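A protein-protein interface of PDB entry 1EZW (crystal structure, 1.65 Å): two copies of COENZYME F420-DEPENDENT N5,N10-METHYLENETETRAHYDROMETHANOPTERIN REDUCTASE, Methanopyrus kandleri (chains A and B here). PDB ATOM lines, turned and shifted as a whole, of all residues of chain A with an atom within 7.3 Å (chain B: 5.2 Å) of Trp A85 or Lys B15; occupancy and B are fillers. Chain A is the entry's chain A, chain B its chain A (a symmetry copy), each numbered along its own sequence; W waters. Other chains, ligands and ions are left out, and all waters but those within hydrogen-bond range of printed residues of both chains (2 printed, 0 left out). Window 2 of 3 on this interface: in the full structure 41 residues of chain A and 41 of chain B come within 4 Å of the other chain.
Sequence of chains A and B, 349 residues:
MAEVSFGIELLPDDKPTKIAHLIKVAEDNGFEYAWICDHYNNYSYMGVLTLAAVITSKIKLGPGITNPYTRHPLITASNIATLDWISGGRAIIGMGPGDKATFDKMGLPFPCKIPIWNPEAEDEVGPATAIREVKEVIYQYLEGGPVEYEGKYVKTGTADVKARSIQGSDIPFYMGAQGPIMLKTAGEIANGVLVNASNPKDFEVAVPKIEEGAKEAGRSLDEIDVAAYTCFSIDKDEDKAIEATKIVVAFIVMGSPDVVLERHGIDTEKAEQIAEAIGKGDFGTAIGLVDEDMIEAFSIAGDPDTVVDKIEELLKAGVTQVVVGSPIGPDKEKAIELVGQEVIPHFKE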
ATOM      1  N   ASN A  79      -4.890   2.968  27.578  1.00  0.00           N
ATOM      2  CA  ASN A  79      -3.424   3.041  27.352  1.00  0.00           C
ATOM      3  C   ASN A  79      -3.123   3.109  25.859  1.00  0.00           C
ATOM      4  O   ASN A  79      -2.375   3.979  25.410  1.00  0.00           O
ATOM      5  CB  ASN A  79      -2.686   1.827  27.897  1.00  0.00           C
ATOM      6  CG  ASN A  79      -2.656   1.801  29.375  1.00  0.00           C
ATOM      7  OD1 ASN A  79      -2.936   2.804  29.997  1.00  0.00           O
ATOM      8  ND2 ASN A  79      -2.280   0.659  29.967  1.00  0.00           N
ATOM      9  N   ILE A  80      -3.717   2.190  25.092  1.00  0.00           N
ATOM     10  CA  ILE A  80      -3.458   2.169  23.657  1.00  0.00           C
ATOM     11  C   ILE A  80      -3.926   3.433  22.959  1.00  0.00           C
ATOM     12  O   ILE A  80      -3.179   3.998  22.116  1.00  0.00           O
ATOM     13  CB  ILE A  80      -4.102   0.907  23.011  1.00  0.00           C
ATOM     14  CG1 ILE A  80      -3.483  -0.333  23.648  1.00  0.00           C
ATOM     15  CG2 ILE A  80      -3.999   0.980  21.486  1.00  0.00           C
ATOM     16  CD1 ILE A  80      -1.978  -0.491  23.416  1.00  0.00           C
ATOM     17  N   ALA A  81      -5.120   3.937  23.288  1.00  0.00           N
ATOM     18  CA  ALA A  81      -5.575   5.147  22.667  1.00  0.00           C
ATOM     19  C   ALA A  81      -4.648   6.336  23.019  1.00  0.00           C
ATOM     20  O   ALA A  81      -4.410   7.205  22.185  1.00  0.00           O
ATOM     21  CB  ALA A  81      -7.014   5.466  23.093  1.00  0.00           C
ATOM     22  N   THR A  82      -4.124   6.330  24.242  1.00  0.00           N
ATOM     23  CA  THR A  82      -3.268   7.442  24.723  1.00  0.00           C
ATOM     24  C   THR A  82      -1.926   7.404  23.994  1.00  0.00           C
ATOM     25  O   THR A  82      -1.466   8.429  23.512  1.00  0.00           O
ATOM     26  CB  THR A  82      -3.097   7.349  26.249  1.00  0.00           C
ATOM     27  OG1 THR A  82      -4.402   7.390  26.852  1.00  0.00           O
ATOM     28  CG2 THR A  82      -2.266   8.558  26.812  1.00  0.00           C
ATOM     29  N   LEU A  83      -1.306   6.221  23.966  1.00  0.00           N
ATOM     30  CA  LEU A  83      -0.044   6.045  23.243  1.00  0.00           C
ATOM     31  C   LEU A  83      -0.267   6.425  21.785  1.00  0.00           C
ATOM     32  O   LEU A  83       0.584   7.085  21.188  1.00  0.00           O
ATOM     33  CB  LEU A  83       0.411   4.602  23.289  1.00  0.00           C
ATOM     34  CG  LEU A  83       1.722   4.283  22.553  1.00  0.00           C
ATOM     35  CD1 LEU A  83       2.885   5.158  23.073  1.00  0.00           C
ATOM     36  CD2 LEU A  83       2.067   2.819  22.814  1.00  0.00           C
ATOM     37  N   ASP A  84      -1.389   6.011  21.181  1.00  0.00           N
ATOM     38  CA  ASP A  84      -1.619   6.367  19.771  1.00  0.00           C
ATOM     39  C   ASP A  84      -1.708   7.886  19.561  1.00  0.00           C
ATOM     40  O   ASP A  84      -1.141   8.449  18.613  1.00  0.00           O
ATOM     41  CB  ASP A  84      -2.934   5.753  19.271  1.00  0.00           C
ATOM     42  CG  ASP A  84      -3.018   5.752  17.770  1.00  0.00           C
ATOM     43  OD1 ASP A  84      -4.008   6.279  17.225  1.00  0.00           O
ATOM     44  OD2 ASP A  84      -2.048   5.223  17.154  1.00  0.00           O
ATOM     45  N   TRP A  85      -2.440   8.562  20.439  1.00  0.00           N
ATOM     46  CA  TRP A  85      -2.596   9.995  20.297  1.00  0.00           C
ATOM     47  C   TRP A  85      -1.238  10.708  20.477  1.00  0.00           C
ATOM     48  O   TRP A  85      -0.833  11.554  19.656  1.00  0.00           O
ATOM     49  CB  TRP A  85      -3.618  10.505  21.336  1.00  0.00           C
ATOM     50  CG  TRP A  85      -4.011  11.930  21.069  1.00  0.00           C
ATOM     51  CD1 TRP A  85      -5.130  12.370  20.372  1.00  0.00           C
ATOM     52  CD2 TRP A  85      -3.290  13.099  21.463  1.00  0.00           C
ATOM     53  NE1 TRP A  85      -5.126  13.757  20.319  1.00  0.00           N
ATOM     54  CE2 TRP A  85      -4.014  14.222  20.976  1.00  0.00           C
ATOM     55  CE3 TRP A  85      -2.094  13.317  22.172  1.00  0.00           C
ATOM     56  CZ2 TRP A  85      -3.578  15.545  21.185  1.00  0.00           C
ATOM     57  CZ3 TRP A  85      -1.655  14.627  22.365  1.00  0.00           C
ATOM     58  CH2 TRP A  85      -2.394  15.726  21.877  1.00  0.00           C
ATOM     59  N   ILE A  86      -0.540  10.405  21.565  1.00  0.00           N
ATOM     60  CA  ILE A  86       0.744  11.047  21.798  1.00  0.00           C
ATOM     61  C   ILE A  86       1.776  10.802  20.692  1.00  0.00           C
ATOM     62  O   ILE A  86       2.543  11.699  20.353  1.00  0.00           O
ATOM     63  CB  ILE A  86       1.311  10.597  23.164  1.00  0.00           C
ATOM     64  CG1 ILE A  86       0.390  11.172  24.266  1.00  0.00           C
ATOM     65  CG2 ILE A  86       2.719  11.190  23.372  1.00  0.00           C
ATOM     66  CD1 ILE A  86       0.713  10.674  25.676  1.00  0.00           C
ATOM     67  N   SER A  87       1.752   9.594  20.096  1.00  0.00           N
ATOM     68  CA  SER A  87       2.705   9.238  19.042  1.00  0.00           C
ATOM     69  C   SER A  87       2.265   9.716  17.656  1.00  0.00           C
ATOM     70  O   SER A  87       2.992   9.472  16.696  1.00  0.00           O
ATOM     71  CB  SER A  87       2.928   7.724  18.986  1.00  0.00           C
ATOM     72  OG  SER A  87       1.733   7.078  18.526  1.00  0.00           O
ATOM     73  N   GLY A  88       1.127  10.388  17.537  1.00  0.00           N
ATOM     74  CA  GLY A  88       0.711  10.855  16.198  1.00  0.00           C
ATOM     75  C   GLY A  88       0.212   9.711  15.302  1.00  0.00           C
ATOM     76  O   GLY A  88       0.364   9.746  14.067  1.00  0.00           O
ATOM     77  N   GLY A  89      -0.359   8.695  15.940  1.00  0.00           N
ATOM     78  CA  GLY A  89      -0.976   7.576  15.226  1.00  0.00           C
ATOM     79  C   GLY A  89      -0.064   6.433  14.869  1.00  0.00           C
ATOM     80  O   GLY A  89      -0.207   5.845  13.756  1.00  0.00           O
ATOM     81  N   ARG A  90       0.823   6.081  15.806  1.00  0.00           N
ATOM     82  CA  ARG A  90       1.795   5.012  15.609  1.00  0.00           C
ATOM     83  C   ARG A  90       1.651   3.800  16.529  1.00  0.00           C
ATOM     84  O   ARG A  90       2.524   2.946  16.554  1.00  0.00           O
ATOM     85  CB  ARG A  90       3.235   5.559  15.752  1.00  0.00           C
ATOM     86  CG  ARG A  90       3.610   6.455  14.595  1.00  0.00           C
ATOM     87  CD  ARG A  90       5.031   6.943  14.768  1.00  0.00           C
ATOM     88  NE  ARG A  90       5.180   7.912  15.862  1.00  0.00           N
ATOM     89  CZ  ARG A  90       6.199   7.889  16.724  1.00  0.00           C
ATOM     90  NH1 ARG A  90       6.279   8.821  17.680  1.00  0.00           N
ATOM     91  NH2 ARG A  90       7.089   6.906  16.690  1.00  0.00           N
ATOM     92  N   ALA A  91       0.571   3.737  17.300  1.00  0.00           N
ATOM     93  CA  ALA A  91       0.421   2.623  18.202  1.00  0.00           C
ATOM     94  C   ALA A  91       0.123   1.295  17.520  1.00  0.00           C
ATOM     95  O   ALA A  91      -0.501   1.262  16.459  1.00  0.00           O
ATOM     96  CB  ALA A  91      -0.697   2.916  19.221  1.00  0.00           C
ATOM     97  N   ALA A 163     -11.625   9.751  25.617  1.00  0.00           N
ATOM     98  CA  ALA A 163     -10.313   9.730  24.944  1.00  0.00           C
ATOM     99  C   ALA A 163     -10.431   9.290  23.501  1.00  0.00           C
ATOM    100  O   ALA A 163     -11.184   8.347  23.181  1.00  0.00           O
ATOM    101  CB  ALA A 163      -9.359   8.789  25.685  1.00  0.00           C
ATOM    102  N   ARG A 164      -9.727   9.988  22.630  1.00  0.00           N
ATOM    103  CA  ARG A 164      -9.732   9.586  21.245  1.00  0.00           C
ATOM    104  C   ARG A 164      -8.307   9.295  20.778  1.00  0.00           C
ATOM    105  O   ARG A 164      -7.349  10.007  21.117  1.00  0.00           O
ATOM    106  CB  ARG A 164     -10.346  10.659  20.349  1.00  0.00           C
ATOM    107  CG  ARG A 164     -11.893  10.740  20.464  1.00  0.00           C
ATOM    108  CD  ARG A 164     -12.568   9.458  19.944  1.00  0.00           C
ATOM    109  NE  ARG A 164     -14.034   9.548  20.035  1.00  0.00           N
ATOM    110  CZ  ARG A 164     -14.737   9.380  21.152  1.00  0.00           C
ATOM    111  NH1 ARG A 164     -16.078   9.490  21.143  1.00  0.00           N
ATOM    112  NH2 ARG A 164     -14.118   9.052  22.271  1.00  0.00           N
ATOM    113  N   SER A 165      -8.176   8.238  19.979  1.00  0.00           N
ATOM    114  CA  SER A 165      -6.896   7.888  19.382  1.00  0.00           C
ATOM    115  C   SER A 165      -6.822   8.622  18.041  1.00  0.00           C
ATOM    116  O   SER A 165      -7.702   9.420  17.728  1.00  0.00           O
ATOM    117  CB  SER A 165      -6.837   6.376  19.111  1.00  0.00           C
ATOM    118  OG  SER A 165      -7.861   6.008  18.174  1.00  0.00           O
ATOM    119  N   ILE A 166      -5.802   8.343  17.244  1.00  0.00           N
ATOM    120  CA  ILE A 166      -5.715   8.964  15.921  1.00  0.00           C
ATOM    121  C   ILE A 166      -6.067   7.931  14.854  1.00  0.00           C
ATOM    122  O   ILE A 166      -6.847   8.221  13.937  1.00  0.00           O
ATOM    123  CB  ILE A 166      -4.319   9.568  15.740  1.00  0.00           C
ATOM    124  CG1 ILE A 166      -4.275  10.841  16.583  1.00  0.00           C
ATOM    125  CG2 ILE A 166      -3.990   9.864  14.228  1.00  0.00           C
ATOM    126  CD1 ILE A 166      -2.942  11.396  16.739  1.00  0.00           C
ATOM    127  N   GLN A 167      -5.553   6.712  14.989  1.00  0.00           N
ATOM    128  CA  GLN A 167      -5.865   5.677  13.987  1.00  0.00           C
ATOM    129  C   GLN A 167      -7.217   5.020  14.227  1.00  0.00           C
ATOM    130  O   GLN A 167      -7.702   4.301  13.344  1.00  0.00           O
ATOM    131  CB  GLN A 167      -4.859   4.537  14.025  1.00  0.00           C
ATOM    132  CG  GLN A 167      -3.440   4.929  13.802  1.00  0.00           C
ATOM    133  CD  GLN A 167      -2.552   3.699  13.844  1.00  0.00           C
ATOM    134  OE1 GLN A 167      -2.443   2.963  12.853  1.00  0.00           O
ATOM    135  NE2 GLN A 167      -1.947   3.432  15.007  1.00  0.00           N
ATOM    136  N   ILE A 171      -5.732   0.787  14.308  1.00  0.00           N
ATOM    137  CA  ILE A 171      -4.593   0.304  15.108  1.00  0.00           C
ATOM    138  C   ILE A 171      -4.495  -1.201  14.926  1.00  0.00           C
ATOM    139  O   ILE A 171      -5.487  -1.917  15.083  1.00  0.00           O
ATOM    140  CB  ILE A 171      -4.795   0.610  16.629  1.00  0.00           C
ATOM    141  CG1 ILE A 171      -4.777   2.122  16.815  1.00  0.00           C
ATOM    142  CG2 ILE A 171      -3.676  -0.050  17.462  1.00  0.00           C
ATOM    143  CD1 ILE A 171      -4.930   2.566  18.307  1.00  0.00           C
ATOM    144  N   ASP B  13      -9.292  14.643  30.153  1.00  0.00           N
ATOM    145  CA  ASP B  13     -10.171  14.356  29.026  1.00  0.00           C
ATOM    146  C   ASP B  13      -9.730  15.203  27.813  1.00  0.00           C
ATOM    147  O   ASP B  13     -10.019  14.871  26.645  1.00  0.00           O
ATOM    148  CB  ASP B  13     -11.651  14.625  29.382  1.00  0.00           C
ATOM    149  CG  ASP B  13     -11.911  16.026  29.922  1.00  0.00           C
ATOM    150  OD1 ASP B  13     -13.102  16.413  29.851  1.00  0.00           O
ATOM    151  OD2 ASP B  13     -11.012  16.750  30.431  1.00  0.00           O
ATOM    152  N   ASP B  14      -8.987  16.256  28.093  1.00  0.00           N
ATOM    153  CA  ASP B  14      -8.542  17.192  27.047  1.00  0.00           C
ATOM    154  C   ASP B  14      -7.293  16.620  26.402  1.00  0.00           C
ATOM    155  O   ASP B  14      -6.772  15.583  26.835  1.00  0.00           O
ATOM    156  CB  ASP B  14      -8.187  18.531  27.683  1.00  0.00           C
ATOM    157  CG  ASP B  14      -8.376  19.730  26.725  1.00  0.00           C
ATOM    158  OD1 ASP B  14      -8.371  19.578  25.485  1.00  0.00           O
ATOM    159  OD2 ASP B  14      -8.502  20.860  27.249  1.00  0.00           O
ATOM    160  N   LYS B  15      -6.820  17.309  25.377  1.00  0.00           N
ATOM    161  CA  LYS B  15      -5.598  16.858  24.688  1.00  0.00           C
ATOM    162  C   LYS B  15      -4.417  16.683  25.662  1.00  0.00           C
ATOM    163  O   LYS B  15      -4.099  17.552  26.468  1.00  0.00           O
ATOM    164  CB  LYS B  15      -5.204  17.888  23.634  1.00  0.00           C
ATOM    165  CG  LYS B  15      -6.302  18.007  22.558  1.00  0.00           C
ATOM    166  CD  LYS B  15      -6.075  19.070  21.549  1.00  0.00           C
ATOM    167  CE  LYS B  15      -7.290  19.170  20.587  1.00  0.00           C
ATOM    168  NZ  LYS B  15      -8.561  19.850  21.102  1.00  0.00           N
ATOM    169  N   PRO B  16      -3.727  15.534  25.595  1.00  0.00           N
ATOM    170  CA  PRO B  16      -2.598  15.337  26.507  1.00  0.00           C
ATOM    171  C   PRO B  16      -1.572  16.461  26.549  1.00  0.00           C
ATOM    172  O   PRO B  16      -1.013  16.773  27.613  1.00  0.00           O
ATOM    173  CB  PRO B  16      -1.999  14.008  26.052  1.00  0.00           C
ATOM    174  CG  PRO B  16      -3.250  13.215  25.700  1.00  0.00           C
ATOM    175  CD  PRO B  16      -4.058  14.272  24.877  1.00  0.00           C
ATOM    176  N   THR B  17      -1.270  17.046  25.386  1.00  0.00           N
ATOM    177  CA  THR B  17      -0.330  18.155  25.322  1.00  0.00           C
ATOM    178  C   THR B  17      -0.893  19.407  26.017  1.00  0.00           C
ATOM    179  O   THR B  17      -0.122  20.233  26.503  1.00  0.00           O
ATOM    180  CB  THR B  17       0.026  18.479  23.859  1.00  0.00           C
ATOM    181  OG1 THR B  17      -1.183  18.585  23.085  1.00  0.00           O
ATOM    182  CG2 THR B  17       0.868  17.386  23.292  1.00  0.00           C
ATOM    183  N   LYS B  18      -2.214  19.587  26.046  1.00  0.00           N
ATOM    184  CA  LYS B  18      -2.778  20.754  26.744  1.00  0.00           C
ATOM    185  C   LYS B  18      -2.657  20.519  28.251  1.00  0.00           C
ATOM    186  O   LYS B  18      -2.259  21.420  29.013  1.00  0.00           O
ATOM    187  CB  LYS B  18      -4.242  20.943  26.355  1.00  0.00           C
ATOM    188  CG  LYS B  18      -5.025  21.947  27.233  1.00  0.00           C
ATOM    189  CD  LYS B  18      -4.420  23.331  27.218  1.00  0.00           C
ATOM    190  CE  LYS B  18      -4.597  24.022  25.885  1.00  0.00           C
ATOM    191  NZ  LYS B  18      -6.020  24.210  25.608  1.00  0.00           N
ATOM    192  N   ILE B  19      -2.958  19.289  28.664  1.00  0.00           N
ATOM    193  CA  ILE B  19      -2.868  18.949  30.080  1.00  0.00           C
ATOM    194  C   ILE B  19      -1.403  19.145  30.512  1.00  0.00           C
ATOM    195  O   ILE B  19      -1.126  19.791  31.545  1.00  0.00           O
ATOM    196  CB  ILE B  19      -3.308  17.486  30.357  1.00  0.00           C
ATOM    197  CG1 ILE B  19      -4.792  17.247  29.991  1.00  0.00           C
ATOM    198  CG2 ILE B  19      -3.068  17.168  31.868  1.00  0.00           C
ATOM    199  CD1 ILE B  19      -5.796  18.182  30.715  1.00  0.00           C
ATOM    200  N   ALA B  20      -0.437  18.633  29.734  1.00  0.00           N
ATOM    201  CA  ALA B  20       0.983  18.832  30.071  1.00  0.00           C
ATOM    202  C   ALA B  20       1.353  20.314  30.128  1.00  0.00           C
ATOM    203  O   ALA B  20       2.053  20.752  31.035  1.00  0.00           O
ATOM    204  CB  ALA B  20       1.873  18.091  29.036  1.00  0.00           C
ATOM    205  N   TYR B  43      -7.822   9.884  28.988  1.00  0.00           N
ATOM    206  CA  TYR B  43      -6.478   9.428  28.617  1.00  0.00           C
ATOM    207  C   TYR B  43      -5.838   8.837  29.893  1.00  0.00           C
ATOM    208  O   TYR B  43      -6.161   9.204  31.025  1.00  0.00           O
ATOM    209  CB  TYR B  43      -5.664  10.583  28.030  1.00  0.00           C
ATOM    210  CG  TYR B  43      -6.147  10.999  26.672  1.00  0.00           C
ATOM    211  CD1 TYR B  43      -6.913  12.158  26.504  1.00  0.00           C
ATOM    212  CD2 TYR B  43      -5.835  10.211  25.542  1.00  0.00           C
ATOM    213  CE1 TYR B  43      -7.370  12.544  25.220  1.00  0.00           C
ATOM    214  CE2 TYR B  43      -6.266  10.571  24.277  1.00  0.00           C
ATOM    215  CZ  TYR B  43      -7.035  11.737  24.123  1.00  0.00           C
ATOM    216  OH  TYR B  43      -7.456  12.076  22.861  1.00  0.00           O
HETATM  217  O   HOH W   1      -7.506  14.840  22.542  1.00  0.00           O
HETATM  218  O   HOH W   2     -10.738  13.033  22.999  1.00  0.00           O
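Printed residues of chain B that touch a printed residue of chain A: Lys B15, Pro B16, Thr B17 and Tyr B43.
Of the 19 printed residues of chain A, 4 touch a printed residue of chain B.
Printed residues of chain A that touch a printed residue of chain B: Thr A82, Trp A85, Ala A163 and Arg A164.
Hydrophobic or aromatic side chains of chain A that line the printed part of chain B: Trp A85 and Ala A163.
Among the printed residues, no Asp or Glu carboxylate lies within 4 Å of a Lys or Arg side-chain nitrogen of the other chain.
Tyr B43 touches Thr A82.
Trp A85 touches Lys B15.
Pro B16 touches Trp A85 (CD to CE3, 3.5 Å).
Thr B17 touches Trp A85.
Tyr B43 touches Trp A85.
Tyr B43 touches Ala A163 (CD2 to CB, 3.8 Å).
Trp A85 touches just these residues of chain B: Lys B15, Pro B16, Thr B17 and Tyr B43.
Lys B15 touches just one residue of chain A: Trp A85 (3.8 Å).
Of the printed residues of chain B, Arg A164 touches Tyr B43 (2.7 Å).
Of the printed residues of chain B, Ala A163 touches Tyr B43.
Ala A91 touches none of the printed residues of chain B.
The nearest printed residue of chain B that does not touch Trp A85 is Lys B18 (5.7 Å).
Water W1 lies within hydrogen-bond range of OH of Tyr B43 (2.8 Å) and NE1 of Trp A85 (3.4 Å).
Water W2 lies within hydrogen-bond range of N of Arg A164 and OH of Tyr B43.
No position is printed for both chains.
Of the 7 pairs that touch across the chains among the printed residues, none has its exchanged pair printed and touching as well.
O of Arg A164 lies within hydrogen-bond range of OH of Tyr B43, 2.7 Å away.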
